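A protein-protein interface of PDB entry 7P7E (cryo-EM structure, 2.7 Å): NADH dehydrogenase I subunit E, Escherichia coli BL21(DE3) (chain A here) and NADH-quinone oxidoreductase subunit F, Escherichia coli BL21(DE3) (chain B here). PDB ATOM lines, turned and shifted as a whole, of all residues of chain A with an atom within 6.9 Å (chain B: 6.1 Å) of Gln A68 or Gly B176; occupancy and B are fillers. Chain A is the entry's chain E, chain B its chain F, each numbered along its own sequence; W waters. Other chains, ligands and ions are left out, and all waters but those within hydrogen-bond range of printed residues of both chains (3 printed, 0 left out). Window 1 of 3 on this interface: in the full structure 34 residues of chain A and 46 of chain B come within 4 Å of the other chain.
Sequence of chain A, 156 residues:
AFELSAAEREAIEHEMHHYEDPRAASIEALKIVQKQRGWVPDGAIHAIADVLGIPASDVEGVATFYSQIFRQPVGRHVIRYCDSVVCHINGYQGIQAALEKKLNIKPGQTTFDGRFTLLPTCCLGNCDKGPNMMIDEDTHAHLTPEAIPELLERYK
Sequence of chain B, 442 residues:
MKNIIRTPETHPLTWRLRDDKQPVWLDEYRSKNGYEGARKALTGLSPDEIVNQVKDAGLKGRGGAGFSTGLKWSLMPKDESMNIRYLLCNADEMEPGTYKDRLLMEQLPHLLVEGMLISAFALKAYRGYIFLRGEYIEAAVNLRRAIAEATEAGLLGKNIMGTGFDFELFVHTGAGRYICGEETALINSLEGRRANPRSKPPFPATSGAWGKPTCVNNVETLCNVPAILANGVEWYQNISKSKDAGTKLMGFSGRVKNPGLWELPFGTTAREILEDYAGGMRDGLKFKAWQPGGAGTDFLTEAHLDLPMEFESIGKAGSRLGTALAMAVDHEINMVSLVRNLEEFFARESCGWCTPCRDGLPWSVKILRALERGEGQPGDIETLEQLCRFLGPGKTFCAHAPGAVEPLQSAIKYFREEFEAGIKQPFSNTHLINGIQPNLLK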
ATOM      1  N   LYS A  31     -34.986   0.432 -21.674  1.00  0.00           N
ATOM      2  CA  LYS A  31     -35.938   0.465 -20.567  1.00  0.00           C
ATOM      3  C   LYS A  31     -37.376   0.284 -21.043  1.00  0.00           C
ATOM      4  O   LYS A  31     -38.180  -0.324 -20.336  1.00  0.00           O
ATOM      5  CB  LYS A  31     -35.790   1.770 -19.789  1.00  0.00           C
ATOM      6  CG  LYS A  31     -34.558   1.807 -18.904  1.00  0.00           C
ATOM      7  CD  LYS A  31     -34.396   3.150 -18.226  1.00  0.00           C
ATOM      8  CE  LYS A  31     -35.316   3.267 -17.027  1.00  0.00           C
ATOM      9  NZ  LYS A  31     -35.028   4.486 -16.229  1.00  0.00           N
ATOM     10  N   GLN A  34     -37.697  -3.386 -21.738  1.00  0.00           N
ATOM     11  CA  GLN A  34     -37.727  -4.072 -20.451  1.00  0.00           C
ATOM     12  C   GLN A  34     -39.074  -3.901 -19.754  1.00  0.00           C
ATOM     13  O   GLN A  34     -39.593  -4.850 -19.161  1.00  0.00           O
ATOM     14  CB  GLN A  34     -36.588  -3.556 -19.572  1.00  0.00           C
ATOM     15  CG  GLN A  34     -36.677  -3.956 -18.115  1.00  0.00           C
ATOM     16  CD  GLN A  34     -35.317  -4.108 -17.477  1.00  0.00           C
ATOM     17  OE1 GLN A  34     -34.505  -4.920 -17.910  1.00  0.00           O
ATOM     18  NE2 GLN A  34     -35.060  -3.320 -16.441  1.00  0.00           N
ATOM     19  N   ALA A  63     -26.344  -2.087 -22.469  1.00  0.00           N
ATOM     20  CA  ALA A  63     -27.262  -2.950 -21.728  1.00  0.00           C
ATOM     21  C   ALA A  63     -26.548  -3.727 -20.630  1.00  0.00           C
ATOM     22  O   ALA A  63     -27.100  -3.920 -19.541  1.00  0.00           O
ATOM     23  CB  ALA A  63     -27.966  -3.908 -22.686  1.00  0.00           C
ATOM     24  N   PHE A  65     -23.671  -2.695 -19.252  1.00  0.00           N
ATOM     25  CA  PHE A  65     -23.062  -1.780 -18.292  1.00  0.00           C
ATOM     26  C   PHE A  65     -24.006  -1.475 -17.133  1.00  0.00           C
ATOM     27  O   PHE A  65     -23.591  -1.488 -15.970  1.00  0.00           O
ATOM     28  CB  PHE A  65     -22.636  -0.486 -18.981  1.00  0.00           C
ATOM     29  CG  PHE A  65     -21.875   0.452 -18.087  1.00  0.00           C
ATOM     30  CD1 PHE A  65     -20.518   0.280 -17.878  1.00  0.00           C
ATOM     31  CD2 PHE A  65     -22.517   1.503 -17.450  1.00  0.00           C
ATOM     32  CE1 PHE A  65     -19.815   1.134 -17.055  1.00  0.00           C
ATOM     33  CE2 PHE A  65     -21.821   2.357 -16.623  1.00  0.00           C
ATOM     34  CZ  PHE A  65     -20.467   2.174 -16.427  1.00  0.00           C
ATOM     35  N   TYR A  66     -25.271  -1.193 -17.428  1.00  0.00           N
ATOM     36  CA  TYR A  66     -26.210  -0.722 -16.420  1.00  0.00           C
ATOM     37  C   TYR A  66     -26.912  -1.901 -15.760  1.00  0.00           C
ATOM     38  O   TYR A  66     -27.385  -2.814 -16.442  1.00  0.00           O
ATOM     39  CB  TYR A  66     -27.225   0.235 -17.041  1.00  0.00           C
ATOM     40  CG  TYR A  66     -26.575   1.477 -17.594  1.00  0.00           C
ATOM     41  CD1 TYR A  66     -26.157   2.498 -16.755  1.00  0.00           C
ATOM     42  CD2 TYR A  66     -26.355   1.617 -18.952  1.00  0.00           C
ATOM     43  CE1 TYR A  66     -25.549   3.624 -17.261  1.00  0.00           C
ATOM     44  CE2 TYR A  66     -25.745   2.732 -19.465  1.00  0.00           C
ATOM     45  CZ  TYR A  66     -25.347   3.735 -18.617  1.00  0.00           C
ATOM     46  OH  TYR A  66     -24.743   4.849 -19.134  1.00  0.00           O
ATOM     47  N   SER A  67     -26.976  -1.868 -14.427  1.00  0.00           N
ATOM     48  CA  SER A  67     -27.457  -3.020 -13.674  1.00  0.00           C
ATOM     49  C   SER A  67     -28.969  -3.180 -13.765  1.00  0.00           C
ATOM     50  O   SER A  67     -29.475  -4.300 -13.637  1.00  0.00           O
ATOM     51  CB  SER A  67     -27.025  -2.903 -12.214  1.00  0.00           C
ATOM     52  OG  SER A  67     -27.588  -1.754 -11.610  1.00  0.00           O
ATOM     53  N   GLN A  68     -29.703  -2.093 -13.981  1.00  0.00           N
ATOM     54  CA  GLN A  68     -31.157  -2.154 -14.002  1.00  0.00           C
ATOM     55  C   GLN A  68     -31.722  -2.514 -15.366  1.00  0.00           C
ATOM     56  O   GLN A  68     -32.944  -2.601 -15.509  1.00  0.00           O
ATOM     57  CB  GLN A  68     -31.756  -0.828 -13.526  1.00  0.00           C
ATOM     58  CG  GLN A  68     -31.524  -0.526 -12.050  1.00  0.00           C
ATOM     59  CD  GLN A  68     -31.494  -1.769 -11.171  1.00  0.00           C
ATOM     60  OE1 GLN A  68     -32.453  -2.546 -11.122  1.00  0.00           O
ATOM     61  NE2 GLN A  68     -30.387  -1.959 -10.461  1.00  0.00           N
ATOM     62  N   ILE A  69     -30.873  -2.724 -16.364  1.00  0.00           N
ATOM     63  CA  ILE A  69     -31.290  -3.292 -17.638  1.00  0.00           C
ATOM     64  C   ILE A  69     -30.957  -4.774 -17.596  1.00  0.00           C
ATOM     65  O   ILE A  69     -29.783  -5.154 -17.519  1.00  0.00           O
ATOM     66  CB  ILE A  69     -30.606  -2.590 -18.821  1.00  0.00           C
ATOM     67  CG1 ILE A  69     -31.143  -1.167 -18.965  1.00  0.00           C
ATOM     68  CG2 ILE A  69     -30.830  -3.368 -20.103  1.00  0.00           C
ATOM     69  CD1 ILE A  69     -30.248  -0.255 -19.765  1.00  0.00           C
ATOM     70  N   PHE A  70     -31.987  -5.612 -17.631  1.00  0.00           N
ATOM     71  CA  PHE A  70     -31.826  -7.040 -17.406  1.00  0.00           C
ATOM     72  C   PHE A  70     -31.640  -7.750 -18.739  1.00  0.00           C
ATOM     73  O   PHE A  70     -32.487  -7.644 -19.630  1.00  0.00           O
ATOM     74  CB  PHE A  70     -33.032  -7.604 -16.657  1.00  0.00           C
ATOM     75  CG  PHE A  70     -33.287  -6.941 -15.335  1.00  0.00           C
ATOM     76  CD1 PHE A  70     -32.233  -6.578 -14.513  1.00  0.00           C
ATOM     77  CD2 PHE A  70     -34.578  -6.680 -14.916  1.00  0.00           C
ATOM     78  CE1 PHE A  70     -32.464  -5.967 -13.299  1.00  0.00           C
ATOM     79  CE2 PHE A  70     -34.814  -6.070 -13.702  1.00  0.00           C
ATOM     80  CZ  PHE A  70     -33.756  -5.713 -12.893  1.00  0.00           C
ATOM     81  N   VAL A  78     -39.617  -8.050  -9.136  1.00  0.00           N
ATOM     82  CA  VAL A  78     -38.206  -7.919  -8.804  1.00  0.00           C
ATOM     83  C   VAL A  78     -38.104  -7.268  -7.433  1.00  0.00           C
ATOM     84  O   VAL A  78     -38.350  -6.067  -7.285  1.00  0.00           O
ATOM     85  CB  VAL A  78     -37.449  -7.105  -9.862  1.00  0.00           C
ATOM     86  CG1 VAL A  78     -35.952  -7.200  -9.631  1.00  0.00           C
ATOM     87  CG2 VAL A  78     -37.813  -7.581 -11.256  1.00  0.00           C
ATOM     88  N   ARG A  80     -35.780  -5.761  -4.765  1.00  0.00           N
ATOM     89  CA  ARG A  80     -34.463  -5.132  -4.758  1.00  0.00           C
ATOM     90  C   ARG A  80     -34.213  -4.571  -3.365  1.00  0.00           C
ATOM     91  O   ARG A  80     -34.721  -3.501  -3.018  1.00  0.00           O
ATOM     92  CB  ARG A  80     -34.374  -4.054  -5.828  1.00  0.00           C
ATOM     93  CG  ARG A  80     -34.205  -4.605  -7.228  1.00  0.00           C
ATOM     94  CD  ARG A  80     -33.452  -3.610  -8.068  1.00  0.00           C
ATOM     95  NE  ARG A  80     -34.212  -2.371  -8.162  1.00  0.00           N
ATOM     96  CZ  ARG A  80     -33.681  -1.167  -8.308  1.00  0.00           C
ATOM     97  NH1 ARG A  80     -32.373  -0.978  -8.275  1.00  0.00           N
ATOM     98  NH2 ARG A  80     -34.485  -0.123  -8.473  1.00  0.00           N
ATOM     99  N   LEU A 119     -32.775  -9.472  -5.644  1.00  0.00           N
ATOM    100  CA  LEU A 119     -31.571  -8.781  -6.058  1.00  0.00           C
ATOM    101  C   LEU A 119     -31.120  -7.810  -4.973  1.00  0.00           C
ATOM    102  O   LEU A 119     -31.939  -7.013  -4.470  1.00  0.00           O
ATOM    103  CB  LEU A 119     -31.792  -8.024  -7.371  1.00  0.00           C
ATOM    104  CG  LEU A 119     -31.956  -8.825  -8.662  1.00  0.00           C
ATOM    105  CD1 LEU A 119     -32.192  -7.888  -9.833  1.00  0.00           C
ATOM    106  CD2 LEU A 119     -30.741  -9.699  -8.909  1.00  0.00           C
ATOM    107  N   PRO A 120     -29.853  -7.857  -4.575  1.00  0.00           N
ATOM    108  CA  PRO A 120     -29.276  -6.726  -3.850  1.00  0.00           C
ATOM    109  C   PRO A 120     -29.128  -5.535  -4.780  1.00  0.00           C
ATOM    110  O   PRO A 120     -28.919  -5.680  -5.986  1.00  0.00           O
ATOM    111  CB  PRO A 120     -27.914  -7.253  -3.391  1.00  0.00           C
ATOM    112  CG  PRO A 120     -27.571  -8.301  -4.385  1.00  0.00           C
ATOM    113  CD  PRO A 120     -28.872  -8.931  -4.800  1.00  0.00           C
ATOM    114  N   THR A 121     -29.245  -4.346  -4.205  1.00  0.00           N
ATOM    115  CA  THR A 121     -29.098  -3.120  -4.968  1.00  0.00           C
ATOM    116  C   THR A 121     -28.386  -2.091  -4.107  1.00  0.00           C
ATOM    117  O   THR A 121     -28.359  -2.189  -2.879  1.00  0.00           O
ATOM    118  CB  THR A 121     -30.452  -2.577  -5.454  1.00  0.00           C
ATOM    119  OG1 THR A 121     -30.234  -1.518  -6.392  1.00  0.00           O
ATOM    120  CG2 THR A 121     -31.284  -2.053  -4.292  1.00  0.00           C
ATOM    121  N   CYS A 122     -27.825  -1.083  -4.768  1.00  0.00           N
ATOM    122  CA  CYS A 122     -27.142  -0.008  -4.070  1.00  0.00           C
ATOM    123  C   CYS A 122     -28.153   0.867  -3.330  1.00  0.00           C
ATOM    124  O   CYS A 122     -29.357   0.592  -3.302  1.00  0.00           O
ATOM    125  CB  CYS A 122     -26.309   0.811  -5.052  1.00  0.00           C
ATOM    126  SG  CYS A 122     -27.213   1.374  -6.507  1.00  0.00           S
ATOM    127  N   MET B  94     -26.639   8.894  -6.069  1.00  0.00           N
ATOM    128  CA  MET B  94     -26.413   7.481  -5.814  1.00  0.00           C
ATOM    129  C   MET B  94     -25.383   7.234  -4.726  1.00  0.00           C
ATOM    130  O   MET B  94     -25.078   6.074  -4.435  1.00  0.00           O
ATOM    131  CB  MET B  94     -25.990   6.774  -7.104  1.00  0.00           C
ATOM    132  CG  MET B  94     -27.155   6.387  -7.982  1.00  0.00           C
ATOM    133  SD  MET B  94     -27.455   4.619  -7.980  1.00  0.00           S
ATOM    134  CE  MET B  94     -28.696   4.509  -9.257  1.00  0.00           C
ATOM    135  N   GLY B 134     -33.293   6.178 -11.841  1.00  0.00           N
ATOM    136  CA  GLY B 134     -34.508   5.452 -12.155  1.00  0.00           C
ATOM    137  C   GLY B 134     -35.295   4.963 -10.963  1.00  0.00           C
ATOM    138  O   GLY B 134     -36.433   4.518 -11.129  1.00  0.00           O
ATOM    139  N   GLU B 135     -34.717   5.037  -9.768  1.00  0.00           N
ATOM    140  CA  GLU B 135     -35.395   4.609  -8.553  1.00  0.00           C
ATOM    141  C   GLU B 135     -36.322   5.674  -7.990  1.00  0.00           C
ATOM    142  O   GLU B 135     -37.095   5.377  -7.074  1.00  0.00           O
ATOM    143  CB  GLU B 135     -34.362   4.217  -7.493  1.00  0.00           C
ATOM    144  CG  GLU B 135     -33.568   2.965  -7.827  1.00  0.00           C
ATOM    145  CD  GLU B 135     -32.389   3.234  -8.745  1.00  0.00           C
ATOM    146  OE1 GLU B 135     -31.991   4.409  -8.870  1.00  0.00           O
ATOM    147  OE2 GLU B 135     -31.871   2.273  -9.348  1.00  0.00           O
ATOM    148  N   GLY B 174     -32.459   7.441 -15.127  1.00  0.00           N
ATOM    149  CA  GLY B 174     -31.255   6.641 -15.137  1.00  0.00           C
ATOM    150  C   GLY B 174     -31.529   5.152 -15.205  1.00  0.00           C
ATOM    151  O   GLY B 174     -32.666   4.685 -15.172  1.00  0.00           O
ATOM    152  N   ALA B 175     -30.437   4.388 -15.295  1.00  0.00           N
ATOM    153  CA  ALA B 175     -30.519   2.938 -15.424  1.00  0.00           C
ATOM    154  C   ALA B 175     -29.685   2.217 -14.371  1.00  0.00           C
ATOM    155  O   ALA B 175     -29.319   1.056 -14.569  1.00  0.00           O
ATOM    156  CB  ALA B 175     -30.100   2.497 -16.827  1.00  0.00           C
ATOM    157  N   GLY B 176     -29.359   2.883 -13.267  1.00  0.00           N
ATOM    158  CA  GLY B 176     -28.831   2.198 -12.104  1.00  0.00           C
ATOM    159  C   GLY B 176     -27.336   1.961 -12.038  1.00  0.00           C
ATOM    160  O   GLY B 176     -26.901   0.813 -11.911  1.00  0.00           O
ATOM    161  N   ARG B 177     -26.539   3.022 -12.113  1.00  0.00           N
ATOM    162  CA  ARG B 177     -25.111   2.935 -11.838  1.00  0.00           C
ATOM    163  C   ARG B 177     -24.681   4.161 -11.048  1.00  0.00           C
ATOM    164  O   ARG B 177     -25.125   5.277 -11.327  1.00  0.00           O
ATOM    165  CB  ARG B 177     -24.280   2.823 -13.124  1.00  0.00           C
ATOM    166  CG  ARG B 177     -24.218   1.425 -13.714  1.00  0.00           C
ATOM    167  CD  ARG B 177     -23.499   0.461 -12.791  1.00  0.00           C
ATOM    168  NE  ARG B 177     -23.408  -0.874 -13.368  1.00  0.00           N
ATOM    169  CZ  ARG B 177     -23.241  -1.985 -12.665  1.00  0.00           C
ATOM    170  NH1 ARG B 177     -23.141  -1.960 -11.346  1.00  0.00           N
ATOM    171  NH2 ARG B 177     -23.177  -3.151 -13.299  1.00  0.00           N
ATOM    172  N   TYR B 178     -23.814   3.944 -10.059  1.00  0.00           N
ATOM    173  CA  TYR B 178     -23.354   5.033  -9.207  1.00  0.00           C
ATOM    174  C   TYR B 178     -22.364   5.943  -9.922  1.00  0.00           C
ATOM    175  O   TYR B 178     -22.314   7.143  -9.634  1.00  0.00           O
ATOM    176  CB  TYR B 178     -22.738   4.459  -7.929  1.00  0.00           C
ATOM    177  CG  TYR B 178     -21.880   5.420  -7.138  1.00  0.00           C
ATOM    178  CD1 TYR B 178     -22.434   6.531  -6.520  1.00  0.00           C
ATOM    179  CD2 TYR B 178     -20.516   5.208  -7.002  1.00  0.00           C
ATOM    180  CE1 TYR B 178     -21.653   7.408  -5.798  1.00  0.00           C
ATOM    181  CE2 TYR B 178     -19.729   6.078  -6.279  1.00  0.00           C
ATOM    182  CZ  TYR B 178     -20.303   7.176  -5.679  1.00  0.00           C
ATOM    183  OH  TYR B 178     -19.522   8.047  -4.958  1.00  0.00           O
ATOM    184  N   CYS B 180     -22.515   7.066 -12.808  1.00  0.00           N
ATOM    185  CA  CYS B 180     -23.244   8.046 -13.609  1.00  0.00           C
ATOM    186  C   CYS B 180     -23.383   9.395 -12.915  1.00  0.00           C
ATOM    187  O   CYS B 180     -23.683  10.388 -13.583  1.00  0.00           O
ATOM    188  CB  CYS B 180     -24.640   7.524 -13.945  1.00  0.00           C
ATOM    189  SG  CYS B 180     -24.677   5.982 -14.847  1.00  0.00           S
ATOM    190  N   GLU B 349     -19.274  -0.825  -8.045  1.00  0.00           N
ATOM    191  CA  GLU B 349     -19.710   0.357  -8.774  1.00  0.00           C
ATOM    192  C   GLU B 349     -18.595   0.979  -9.602  1.00  0.00           C
ATOM    193  O   GLU B 349     -18.773   2.076 -10.137  1.00  0.00           O
ATOM    194  CB  GLU B 349     -20.298   1.384  -7.812  1.00  0.00           C
ATOM    195  CG  GLU B 349     -21.659   0.988  -7.287  1.00  0.00           C
ATOM    196  CD  GLU B 349     -22.645   0.643  -8.388  1.00  0.00           C
ATOM    197  OE1 GLU B 349     -22.770   1.424  -9.354  1.00  0.00           O
ATOM    198  OE2 GLU B 349     -23.300  -0.414  -8.286  1.00  0.00           O
HETATM  199  O   HOH W   1     -29.858   1.448  -6.889  1.00  0.00           O
HETATM  200  O   HOH W   2     -26.114  -0.233  -9.742  1.00  0.00           O
HETATM  201  O   HOH W   3     -26.674   4.119  -5.054  1.00  0.00           O
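The side-chain sulfur of Met B94 sits at hydrogen-bond distance from the side-chain sulfur of Cys A122, at 3.6 Å.
OE2 of Glu B135 lies within salt-bridge range of NH1 of Arg A80.
The side-chain amino group (NZ) of Lys A31 is in hydrogen-bond range of the backbone carbonyl oxygen (O) of Gly B174 (2.6 Å).
O of Ala B175 sits at hydrogen-bond distance from N of Gln A68 (3.2 Å).
The backbone carbonyl oxygen of Gly B176 sits at hydrogen-bond distance from the side-chain hydroxyl of Ser A67 (2.7 Å).
O of Phe A65 lies within hydrogen-bond range of NE of Arg B177.
The side-chain sulfur (SG) of Cys B180 lies close to the backbone carbonyl oxygen (O) of Arg B177, at 3.6 Å.
The side-chain carboxylate (OE2) of Glu B349 lies within salt-bridge range of the guanidinium group (NH1) of Arg B177.
O of Gln A68 sits at hydrogen-bond distance from NE2 of Gln A34 (2.4 Å).
The side-chain hydroxyl (OG) of Ser A67 lies within hydrogen-bond range of the side-chain amide nitrogen (NE2) of Gln A68, at 3.0 Å.
The side-chain amide nitrogen of Gln A68 lies close to the guanidinium group of Arg A80 (3.1 Å).
NH1 of Arg A80 lies within hydrogen-bond range of OG1 of Thr A121.
Among the printed residues, pairs that only touch across the chains: Tyr A66 with Ala B175 (3.3 Å), Tyr A66 with Arg B177 (3.8 Å), Tyr A66 with Cys B180 (3.5 Å), Ser A67 with Ala B175 (3.7 Å), Ser A67 with Arg B177 (3.9 Å), Gln A68 with Glu B135 (3.9 Å) and Gln A68 with Gly B176 (3.8 Å).
Printed residues of chain B within 4 Å of Phe A65: Arg B177 (2.7 Å).
Of the printed residues of chain B, Tyr A66 touches Ala B175 (3.3 Å), Arg B177 (3.8 Å) and Cys B180 (3.5 Å).
Of the printed residues of chain B, Ser A67 touches Ala B175, Gly B176 and Arg B177.
Thr A121 touches none of the printed residues of chain B.
Of the printed residues of chain A, Gly B174 touches Lys A31.
Gly B176 touches just these residues of chain A: Ser A67 and Gln A68.
Printed residues of chain A within 4 Å of Cys B180: Tyr A66 (3.5 Å).
The nearest residue of chain B that does not touch Gln A68 is Gly B174 (5.8 Å).
Hydrophobic or aromatic side chains of chain B that line the printed part of chain A: Met B94 and Ala B175.
Hydrophobic or aromatic side chains of chain A that line the printed part of chain B: Phe A65 and Tyr A66.
Among the printed residues, Asp or Glu carboxylates within 4 Å of a Lys or Arg side-chain nitrogen of the other chain: Arg A80 with Glu B135.
Water W2 lies within hydrogen-bond range of the backbone carbonyl oxygen of Gly B176, the side-chain hydroxyl of Ser A67, the side-chain carboxylate of Glu B349 and the side-chain sulfur of Cys A122.
Water W3 bridges O of Met B94 (2.6 Å) and SG of Cys A122 (3.2 Å).
Water W1 lies within hydrogen-bond range of the side-chain sulfur (SG) of Cys A122, the side-chain hydroxyl (OG1) of Thr A121 and the side-chain carboxylate (OE2) of Glu B135.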
